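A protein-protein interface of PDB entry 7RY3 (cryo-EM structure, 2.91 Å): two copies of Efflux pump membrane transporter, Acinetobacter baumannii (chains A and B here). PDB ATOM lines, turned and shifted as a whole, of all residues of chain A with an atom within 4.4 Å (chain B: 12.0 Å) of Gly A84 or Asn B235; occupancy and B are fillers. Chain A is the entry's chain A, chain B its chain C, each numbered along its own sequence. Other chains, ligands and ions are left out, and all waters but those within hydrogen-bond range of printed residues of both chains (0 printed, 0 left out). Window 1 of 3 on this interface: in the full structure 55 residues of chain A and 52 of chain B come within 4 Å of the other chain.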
ATOM      1  N   GLY A  51      31.109 -12.157 -30.602  1.00  0.00           N
ATOM      2  CA  GLY A  51      29.673 -11.968 -30.663  1.00  0.00           C
ATOM      3  C   GLY A  51      28.898 -13.219 -30.945  1.00  0.00           C
ATOM      4  O   GLY A  51      27.685 -13.175 -31.064  1.00  0.00           O
ATOM      5  N   ALA A  52      29.570 -14.352 -31.010  1.00  0.00           N
ATOM      6  CA  ALA A  52      28.899 -15.570 -31.393  1.00  0.00           C
ATOM      7  C   ALA A  52      28.638 -16.550 -30.270  1.00  0.00           C
ATOM      8  O   ALA A  52      29.384 -16.612 -29.298  1.00  0.00           O
ATOM      9  CB  ALA A  52      29.646 -16.239 -32.536  1.00  0.00           C
ATOM     10  N   SER A  53      27.552 -17.294 -30.387  1.00  0.00           N
ATOM     11  CA  SER A  53      27.179 -18.277 -29.392  1.00  0.00           C
ATOM     12  C   SER A  53      27.974 -19.557 -29.456  1.00  0.00           C
ATOM     13  O   SER A  53      28.662 -19.807 -30.435  1.00  0.00           O
ATOM     14  CB  SER A  53      25.714 -18.624 -29.590  1.00  0.00           C
ATOM     15  OG  SER A  53      25.512 -19.326 -30.802  1.00  0.00           O
ATOM     16  N   ALA A  54      27.853 -20.390 -28.431  1.00  0.00           N
ATOM     17  CA  ALA A  54      28.581 -21.641 -28.376  1.00  0.00           C
ATOM     18  C   ALA A  54      28.171 -22.540 -29.520  1.00  0.00           C
ATOM     19  O   ALA A  54      28.943 -23.377 -29.962  1.00  0.00           O
ATOM     20  CB  ALA A  54      28.307 -22.326 -27.055  1.00  0.00           C
ATOM     21  N   ALA A  83      32.745 -21.940 -26.909  1.00  0.00           N
ATOM     22  CA  ALA A  83      32.166 -21.160 -25.812  1.00  0.00           C
ATOM     23  C   ALA A  83      31.381 -19.904 -26.154  1.00  0.00           C
ATOM     24  O   ALA A  83      31.555 -19.337 -27.223  1.00  0.00           O
ATOM     25  CB  ALA A  83      33.277 -20.808 -24.854  1.00  0.00           C
ATOM     26  N   GLY A  84      30.468 -19.507 -25.276  1.00  0.00           N
ATOM     27  CA  GLY A  84      29.610 -18.350 -25.499  1.00  0.00           C
ATOM     28  C   GLY A  84      30.283 -17.011 -25.620  1.00  0.00           C
ATOM     29  O   GLY A  84      29.675 -16.070 -26.101  1.00  0.00           O
ATOM     30  N   ASN A  85      31.524 -16.901 -25.176  1.00  0.00           N
ATOM     31  CA  ASN A  85      32.261 -15.678 -25.360  1.00  0.00           C
ATOM     32  C   ASN A  85      32.811 -15.573 -26.783  1.00  0.00           C
ATOM     33  O   ASN A  85      33.296 -14.520 -27.175  1.00  0.00           O
ATOM     34  CB  ASN A  85      33.402 -15.633 -24.359  1.00  0.00           C
ATOM     35  CG  ASN A  85      34.332 -16.828 -24.451  1.00  0.00           C
ATOM     36  OD1 ASN A  85      34.110 -17.759 -25.214  1.00  0.00           O
ATOM     37  ND2 ASN A  85      35.390 -16.798 -23.659  1.00  0.00           N
ATOM     38  N   GLY A  86      32.766 -16.657 -27.556  1.00  0.00           N
ATOM     39  CA  GLY A  86      33.181 -16.641 -28.942  1.00  0.00           C
ATOM     40  C   GLY A  86      34.435 -17.430 -29.157  1.00  0.00           C
ATOM     41  O   GLY A  86      34.894 -17.574 -30.279  1.00  0.00           O
ATOM     42  N   TYR A 728      21.800 -13.366 -21.123  1.00  0.00           N
ATOM     43  CA  TYR A 728      20.960 -12.216 -21.452  1.00  0.00           C
ATOM     44  C   TYR A 728      20.945 -11.967 -22.934  1.00  0.00           C
ATOM     45  O   TYR A 728      21.948 -11.590 -23.514  1.00  0.00           O
ATOM     46  CB  TYR A 728      21.364 -10.955 -20.703  1.00  0.00           C
ATOM     47  CG  TYR A 728      20.276  -9.913 -20.741  1.00  0.00           C
ATOM     48  CD1 TYR A 728      19.089 -10.110 -20.058  1.00  0.00           C
ATOM     49  CD2 TYR A 728      20.420  -8.753 -21.479  1.00  0.00           C
ATOM     50  CE1 TYR A 728      18.081  -9.173 -20.095  1.00  0.00           C
ATOM     51  CE2 TYR A 728      19.419  -7.810 -21.522  1.00  0.00           C
ATOM     52  CZ  TYR A 728      18.252  -8.025 -20.830  1.00  0.00           C
ATOM     53  OH  TYR A 728      17.257  -7.084 -20.873  1.00  0.00           O
ATOM     54  N   GLN A 729      19.790 -12.171 -23.556  1.00  0.00           N
ATOM     55  CA  GLN A 729      19.713 -12.046 -25.002  1.00  0.00           C
ATOM     56  C   GLN A 729      19.085 -10.771 -25.443  1.00  0.00           C
ATOM     57  O   GLN A 729      17.999 -10.431 -25.006  1.00  0.00           O
ATOM     58  CB  GLN A 729      18.975 -13.222 -25.620  1.00  0.00           C
ATOM     59  CG  GLN A 729      19.098 -13.283 -27.134  1.00  0.00           C
ATOM     60  CD  GLN A 729      18.611 -14.594 -27.709  1.00  0.00           C
ATOM     61  OE1 GLN A 729      18.367 -15.551 -26.977  1.00  0.00           O
ATOM     62  NE2 GLN A 729      18.475 -14.648 -29.029  1.00  0.00           N
ATOM     63  N   ILE A 730      19.780 -10.054 -26.309  1.00  0.00           N
ATOM     64  CA  ILE A 730      19.293  -8.800 -26.794  1.00  0.00           C
ATOM     65  C   ILE A 730      18.898  -9.040 -28.223  1.00  0.00           C
ATOM     66  O   ILE A 730      19.652  -9.635 -28.983  1.00  0.00           O
ATOM     67  CB  ILE A 730      20.395  -7.728 -26.723  1.00  0.00           C
ATOM     68  CG1 ILE A 730      20.492  -7.163 -25.315  1.00  0.00           C
ATOM     69  CG2 ILE A 730      20.115  -6.582 -27.678  1.00  0.00           C
ATOM     70  CD1 ILE A 730      19.323  -6.279 -24.950  1.00  0.00           C
ATOM     71  N   PRO A 815      26.928 -22.522 -21.586  1.00  0.00           N
ATOM     72  CA  PRO A 815      28.105 -21.665 -21.703  1.00  0.00           C
ATOM     73  C   PRO A 815      29.212 -22.236 -22.612  1.00  0.00           C
ATOM     74  O   PRO A 815      29.836 -21.448 -23.295  1.00  0.00           O
ATOM     75  CB  PRO A 815      28.533 -21.494 -20.255  1.00  0.00           C
ATOM     76  CG  PRO A 815      28.124 -22.757 -19.610  1.00  0.00           C
ATOM     77  CD  PRO A 815      26.813 -23.107 -20.244  1.00  0.00           C
ATOM     78  N   SER B 212      25.166  -7.260 -40.039  1.00  0.00           N
ATOM     79  CA  SER B 212      26.300  -7.282 -39.104  1.00  0.00           C
ATOM     80  C   SER B 212      26.141  -8.120 -37.828  1.00  0.00           C
ATOM     81  O   SER B 212      25.025  -8.302 -37.367  1.00  0.00           O
ATOM     82  CB  SER B 212      26.593  -5.831 -38.697  1.00  0.00           C
ATOM     83  OG  SER B 212      27.642  -5.760 -37.748  1.00  0.00           O
ATOM     84  N   GLN B 213      27.231  -8.606 -37.226  1.00  0.00           N
ATOM     85  CA  GLN B 213      27.098  -9.268 -35.920  1.00  0.00           C
ATOM     86  C   GLN B 213      27.522  -8.388 -34.789  1.00  0.00           C
ATOM     87  O   GLN B 213      28.701  -8.117 -34.632  1.00  0.00           O
ATOM     88  CB  GLN B 213      27.850 -10.591 -35.837  1.00  0.00           C
ATOM     89  CG  GLN B 213      27.450 -11.403 -34.619  1.00  0.00           C
ATOM     90  CD  GLN B 213      28.027 -12.794 -34.631  1.00  0.00           C
ATOM     91  OE1 GLN B 213      29.169 -12.996 -35.021  1.00  0.00           O
ATOM     92  NE2 GLN B 213      27.237 -13.765 -34.196  1.00  0.00           N
ATOM     93  N   VAL B 214      26.564  -7.976 -33.975  1.00  0.00           N
ATOM     94  CA  VAL B 214      26.833  -7.137 -32.824  1.00  0.00           C
ATOM     95  C   VAL B 214      27.490  -7.910 -31.704  1.00  0.00           C
ATOM     96  O   VAL B 214      27.134  -9.052 -31.432  1.00  0.00           O
ATOM     97  CB  VAL B 214      25.528  -6.454 -32.347  1.00  0.00           C
ATOM     98  CG1 VAL B 214      25.755  -5.599 -31.109  1.00  0.00           C
ATOM     99  CG2 VAL B 214      24.946  -5.601 -33.459  1.00  0.00           C
ATOM    100  N   ALA B 215      28.453  -7.293 -31.046  1.00  0.00           N
ATOM    101  CA  ALA B 215      29.113  -7.924 -29.941  1.00  0.00           C
ATOM    102  C   ALA B 215      29.004  -6.882 -28.872  1.00  0.00           C
ATOM    103  O   ALA B 215      29.202  -5.709 -29.149  1.00  0.00           O
ATOM    104  CB  ALA B 215      30.553  -8.190 -30.277  1.00  0.00           C
ATOM    105  N   VAL B 216      28.625  -7.283 -27.667  1.00  0.00           N
ATOM    106  CA  VAL B 216      28.430  -6.346 -26.574  1.00  0.00           C
ATOM    107  C   VAL B 216      29.440  -6.569 -25.439  1.00  0.00           C
ATOM    108  O   VAL B 216      30.410  -5.828 -25.348  1.00  0.00           O
ATOM    109  CB  VAL B 216      26.992  -6.445 -26.031  1.00  0.00           C
ATOM    110  CG1 VAL B 216      26.670  -5.268 -25.129  1.00  0.00           C
ATOM    111  CG2 VAL B 216      25.991  -6.529 -27.170  1.00  0.00           C
ATOM    112  N   GLY B 217      29.207  -7.545 -24.570  1.00  0.00           N
ATOM    113  CA  GLY B 217      30.086  -7.807 -23.433  1.00  0.00           C
ATOM    114  C   GLY B 217      29.506  -8.723 -22.364  1.00  0.00           C
ATOM    115  O   GLY B 217      28.961  -9.774 -22.681  1.00  0.00           O
ATOM    116  N   GLN B 218      29.577  -8.315 -21.095  1.00  0.00           N
ATOM    117  CA  GLN B 218      29.026  -9.098 -19.989  1.00  0.00           C
ATOM    118  C   GLN B 218      28.417  -8.176 -18.960  1.00  0.00           C
ATOM    119  O   GLN B 218      28.864  -7.061 -18.797  1.00  0.00           O
ATOM    120  CB  GLN B 218      30.125  -9.886 -19.273  1.00  0.00           C
ATOM    121  CG  GLN B 218      30.706 -11.053 -20.037  1.00  0.00           C
ATOM    122  CD  GLN B 218      31.817 -11.709 -19.260  1.00  0.00           C
ATOM    123  OE1 GLN B 218      32.086 -11.333 -18.126  1.00  0.00           O
ATOM    124  NE2 GLN B 218      32.462 -12.697 -19.860  1.00  0.00           N
ATOM    125  N   LEU B 219      27.352  -8.625 -18.308  1.00  0.00           N
ATOM    126  CA  LEU B 219      26.682  -7.830 -17.294  1.00  0.00           C
ATOM    127  C   LEU B 219      27.513  -7.535 -16.072  1.00  0.00           C
ATOM    128  O   LEU B 219      27.558  -6.406 -15.605  1.00  0.00           O
ATOM    129  CB  LEU B 219      25.403  -8.522 -16.837  1.00  0.00           C
ATOM    130  CG  LEU B 219      24.199  -8.570 -17.767  1.00  0.00           C
ATOM    131  CD1 LEU B 219      23.100  -9.389 -17.127  1.00  0.00           C
ATOM    132  CD2 LEU B 219      23.704  -7.171 -18.052  1.00  0.00           C
ATOM    133  N   GLY B 220      28.208  -8.530 -15.564  1.00  0.00           N
ATOM    134  CA  GLY B 220      28.971  -8.318 -14.363  1.00  0.00           C
ATOM    135  C   GLY B 220      30.109  -7.396 -14.603  1.00  0.00           C
ATOM    136  O   GLY B 220      30.198  -6.392 -13.946  1.00  0.00           O
ATOM    137  N   ASN B 231      26.753 -12.102 -12.878  1.00  0.00           N
ATOM    138  CA  ASN B 231      27.544 -11.919 -14.077  1.00  0.00           C
ATOM    139  C   ASN B 231      26.899 -12.764 -15.115  1.00  0.00           C
ATOM    140  O   ASN B 231      26.652 -13.923 -14.852  1.00  0.00           O
ATOM    141  CB  ASN B 231      29.001 -12.337 -13.886  1.00  0.00           C
ATOM    142  CG  ASN B 231      29.846 -12.106 -15.117  1.00  0.00           C
ATOM    143  OD1 ASN B 231      29.599 -11.190 -15.893  1.00  0.00           O
ATOM    144  ND2 ASN B 231      30.859 -12.938 -15.298  1.00  0.00           N
ATOM    145  N   ALA B 232      26.585 -12.210 -16.275  1.00  0.00           N
ATOM    146  CA  ALA B 232      26.110 -13.033 -17.361  1.00  0.00           C
ATOM    147  C   ALA B 232      26.775 -12.610 -18.649  1.00  0.00           C
ATOM    148  O   ALA B 232      27.698 -11.837 -18.633  1.00  0.00           O
ATOM    149  CB  ALA B 232      24.612 -12.987 -17.453  1.00  0.00           C
ATOM    150  N   THR B 233      26.275 -13.088 -19.772  1.00  0.00           N
ATOM    151  CA  THR B 233      26.840 -12.740 -21.060  1.00  0.00           C
ATOM    152  C   THR B 233      25.760 -12.076 -21.880  1.00  0.00           C
ATOM    153  O   THR B 233      24.639 -12.565 -21.937  1.00  0.00           O
ATOM    154  CB  THR B 233      27.362 -13.980 -21.805  1.00  0.00           C
ATOM    155  OG1 THR B 233      28.276 -14.695 -20.969  1.00  0.00           O
ATOM    156  CG2 THR B 233      28.076 -13.584 -23.086  1.00  0.00           C
ATOM    157  N   VAL B 234      26.036 -10.852 -22.317  1.00  0.00           N
ATOM    158  CA  VAL B 234      25.235 -10.247 -23.354  1.00  0.00           C
ATOM    159  C   VAL B 234      25.541 -10.545 -24.780  1.00  0.00           C
ATOM    160  O   VAL B 234      26.640 -10.295 -25.264  1.00  0.00           O
ATOM    161  CB  VAL B 234      25.171  -8.721 -23.102  1.00  0.00           C
ATOM    162  CG1 VAL B 234      23.818  -8.197 -23.551  1.00  0.00           C
ATOM    163  CG2 VAL B 234      25.396  -8.424 -21.627  1.00  0.00           C
ATOM    164  N   ASN B 235      24.537 -11.053 -25.482  1.00  0.00           N
ATOM    165  CA  ASN B 235      24.712 -11.421 -26.860  1.00  0.00           C
ATOM    166  C   ASN B 235      23.590 -10.847 -27.674  1.00  0.00           C
ATOM    167  O   ASN B 235      22.457 -10.805 -27.228  1.00  0.00           O
ATOM    168  CB  ASN B 235      24.743 -12.925 -27.013  1.00  0.00           C
ATOM    169  CG  ASN B 235      26.148 -13.462 -27.179  1.00  0.00           C
ATOM    170  OD1 ASN B 235      27.127 -12.736 -27.038  1.00  0.00           O
ATOM    171  ND2 ASN B 235      26.251 -14.750 -27.491  1.00  0.00           N
ATOM    172  N   ALA B 236      23.903 -10.386 -28.874  1.00  0.00           N
ATOM    173  CA  ALA B 236      22.888  -9.801 -29.731  1.00  0.00           C
ATOM    174  C   ALA B 236      22.752 -10.594 -31.001  1.00  0.00           C
ATOM    175  O   ALA B 236      23.746 -10.826 -31.681  1.00  0.00           O
ATOM    176  CB  ALA B 236      23.237  -8.361 -30.041  1.00  0.00           C
ATOM    177  N   GLN B 237      21.555 -11.074 -31.322  1.00  0.00           N
ATOM    178  CA  GLN B 237      21.393 -11.724 -32.622  1.00  0.00           C
ATOM    179  C   GLN B 237      20.959 -10.626 -33.545  1.00  0.00           C
ATOM    180  O   GLN B 237      19.925 -10.005 -33.334  1.00  0.00           O
ATOM    181  CB  GLN B 237      20.320 -12.806 -32.565  1.00  0.00           C
ATOM    182  CG  GLN B 237      20.045 -13.472 -33.900  1.00  0.00           C
ATOM    183  CD  GLN B 237      18.804 -14.337 -33.866  1.00  0.00           C
ATOM    184  OE1 GLN B 237      18.237 -14.586 -32.802  1.00  0.00           O
ATOM    185  NE2 GLN B 237      18.381 -14.808 -35.031  1.00  0.00           N
ATOM    186  N   SER B 238      21.742 -10.378 -34.578  1.00  0.00           N
ATOM    187  CA  SER B 238      21.452  -9.281 -35.478  1.00  0.00           C
ATOM    188  C   SER B 238      21.631  -9.637 -36.956  1.00  0.00           C
ATOM    189  O   SER B 238      21.234  -8.872 -37.821  1.00  0.00           O
ATOM    190  CB  SER B 238      22.346  -8.118 -35.092  1.00  0.00           C
ATOM    191  OG  SER B 238      23.639  -8.574 -34.755  1.00  0.00           O
ATOM    192  N   LEU B 239      22.214 -10.793 -37.241  1.00  0.00           N
ATOM    193  CA  LEU B 239      22.460 -11.200 -38.616  1.00  0.00           C
ATOM    194  C   LEU B 239      21.207 -11.646 -39.353  1.00  0.00           C
ATOM    195  O   LEU B 239      20.202 -11.983 -38.735  1.00  0.00           O
ATOM    196  CB  LEU B 239      23.534 -12.283 -38.699  1.00  0.00           C
ATOM    197  CG  LEU B 239      25.005 -11.937 -38.490  1.00  0.00           C
ATOM    198  CD1 LEU B 239      25.768 -13.166 -38.030  1.00  0.00           C
ATOM    199  CD2 LEU B 239      25.609 -11.390 -39.767  1.00  0.00           C
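Of chain B, only Gln B213 (3.2 Å), Val B214 (3.9 Å) and Ala B215 (3.9 Å) come within 4 Å of Gly A51. Of chain B, only Gln B213 comes within 4 Å of Ala A52. No residue of chain B comes within 4 Å of Ala A83. Of the printed residues of chain B, Gly A84 touches Asn B235 (3.9 Å). No residue of chain B comes within 4 Å of Asn A85. Gln A729 touches just these residues of chain B: Asn B235 (3.7 Å) and Gln B237 (3.8 Å). No residue of chain B comes within 4 Å of Pro A815. Of the printed residues of chain A, Val B214 touches Gly A51 (3.9 Å). Asn B235 touches four residues of chain A. Of the printed residues of chain A, Ala B236 touches Ile A730. The nearest printed residue of chain A that does not touch Asn B235 is Ala A52 (4.1 Å).
The side-chain amide nitrogen of Gln B213 is in hydrogen-bond range of the backbone carbonyl oxygen of Gly A51 (3.2 Å). The backbone NH of Asn B235 is in hydrogen-bond range of the backbone carbonyl oxygen of Tyr A728 (3.3 Å). N of Tyr A728 is in hydrogen-bond range of O of Thr B233 (3.1 Å). The backbone NH (N) of Gln B237 lies within hydrogen-bond range of the backbone carbonyl oxygen (O) of Ile A730 (3.3 Å). The backbone NH (N) of Ile A730 lies within hydrogen-bond range of the backbone carbonyl oxygen (O) of Asn B235 (2.9 Å).
Hydrophobic or aromatic side chains of chain A that line the printed part of chain B: Ala A52, Tyr A728 and Ile A730. Hydrophobic or aromatic side chains of chain B that line the printed part of chain A: Ala B215, Val B234 and Ala B236. Among the printed residues, no Asp or Glu carboxylate lies within 4 Å of a Lys or Arg side-chain nitrogen of the other chain.
The backbone NH of Gly A84 sits at hydrogen-bond distance from the backbone carbonyl oxygen of Pro A815. The backbone NH (N) of Val B214 sits at hydrogen-bond distance from the side-chain hydroxyl (OG) of Ser B238 (3.1 Å). N of Val B234 sits at hydrogen-bond distance from O of Gly B217.
No position is printed for both chains. Of the 14 pairs that touch across the chains among the printed residues, none has its exchanged pair printed and touching as well.
Among the printed residues, merely in contact across the chains: Ile A730 with Ala B236 (3.3 Å), Tyr A728 with Val B234 (3.6 Å), Ala A52 with Gln B213 (3.7 Å), Gln A729 with Asn B235 (3.7 Å), Gln A729 with Gln B237 (3.8 Å), Gly A51 with Ala B215 (3.9 Å), Ile A730 with Val B234 (3.9 Å), Gly A84 with Asn B235 (3.9 Å) and Gly A51 with Val B214 (3.9 Å).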
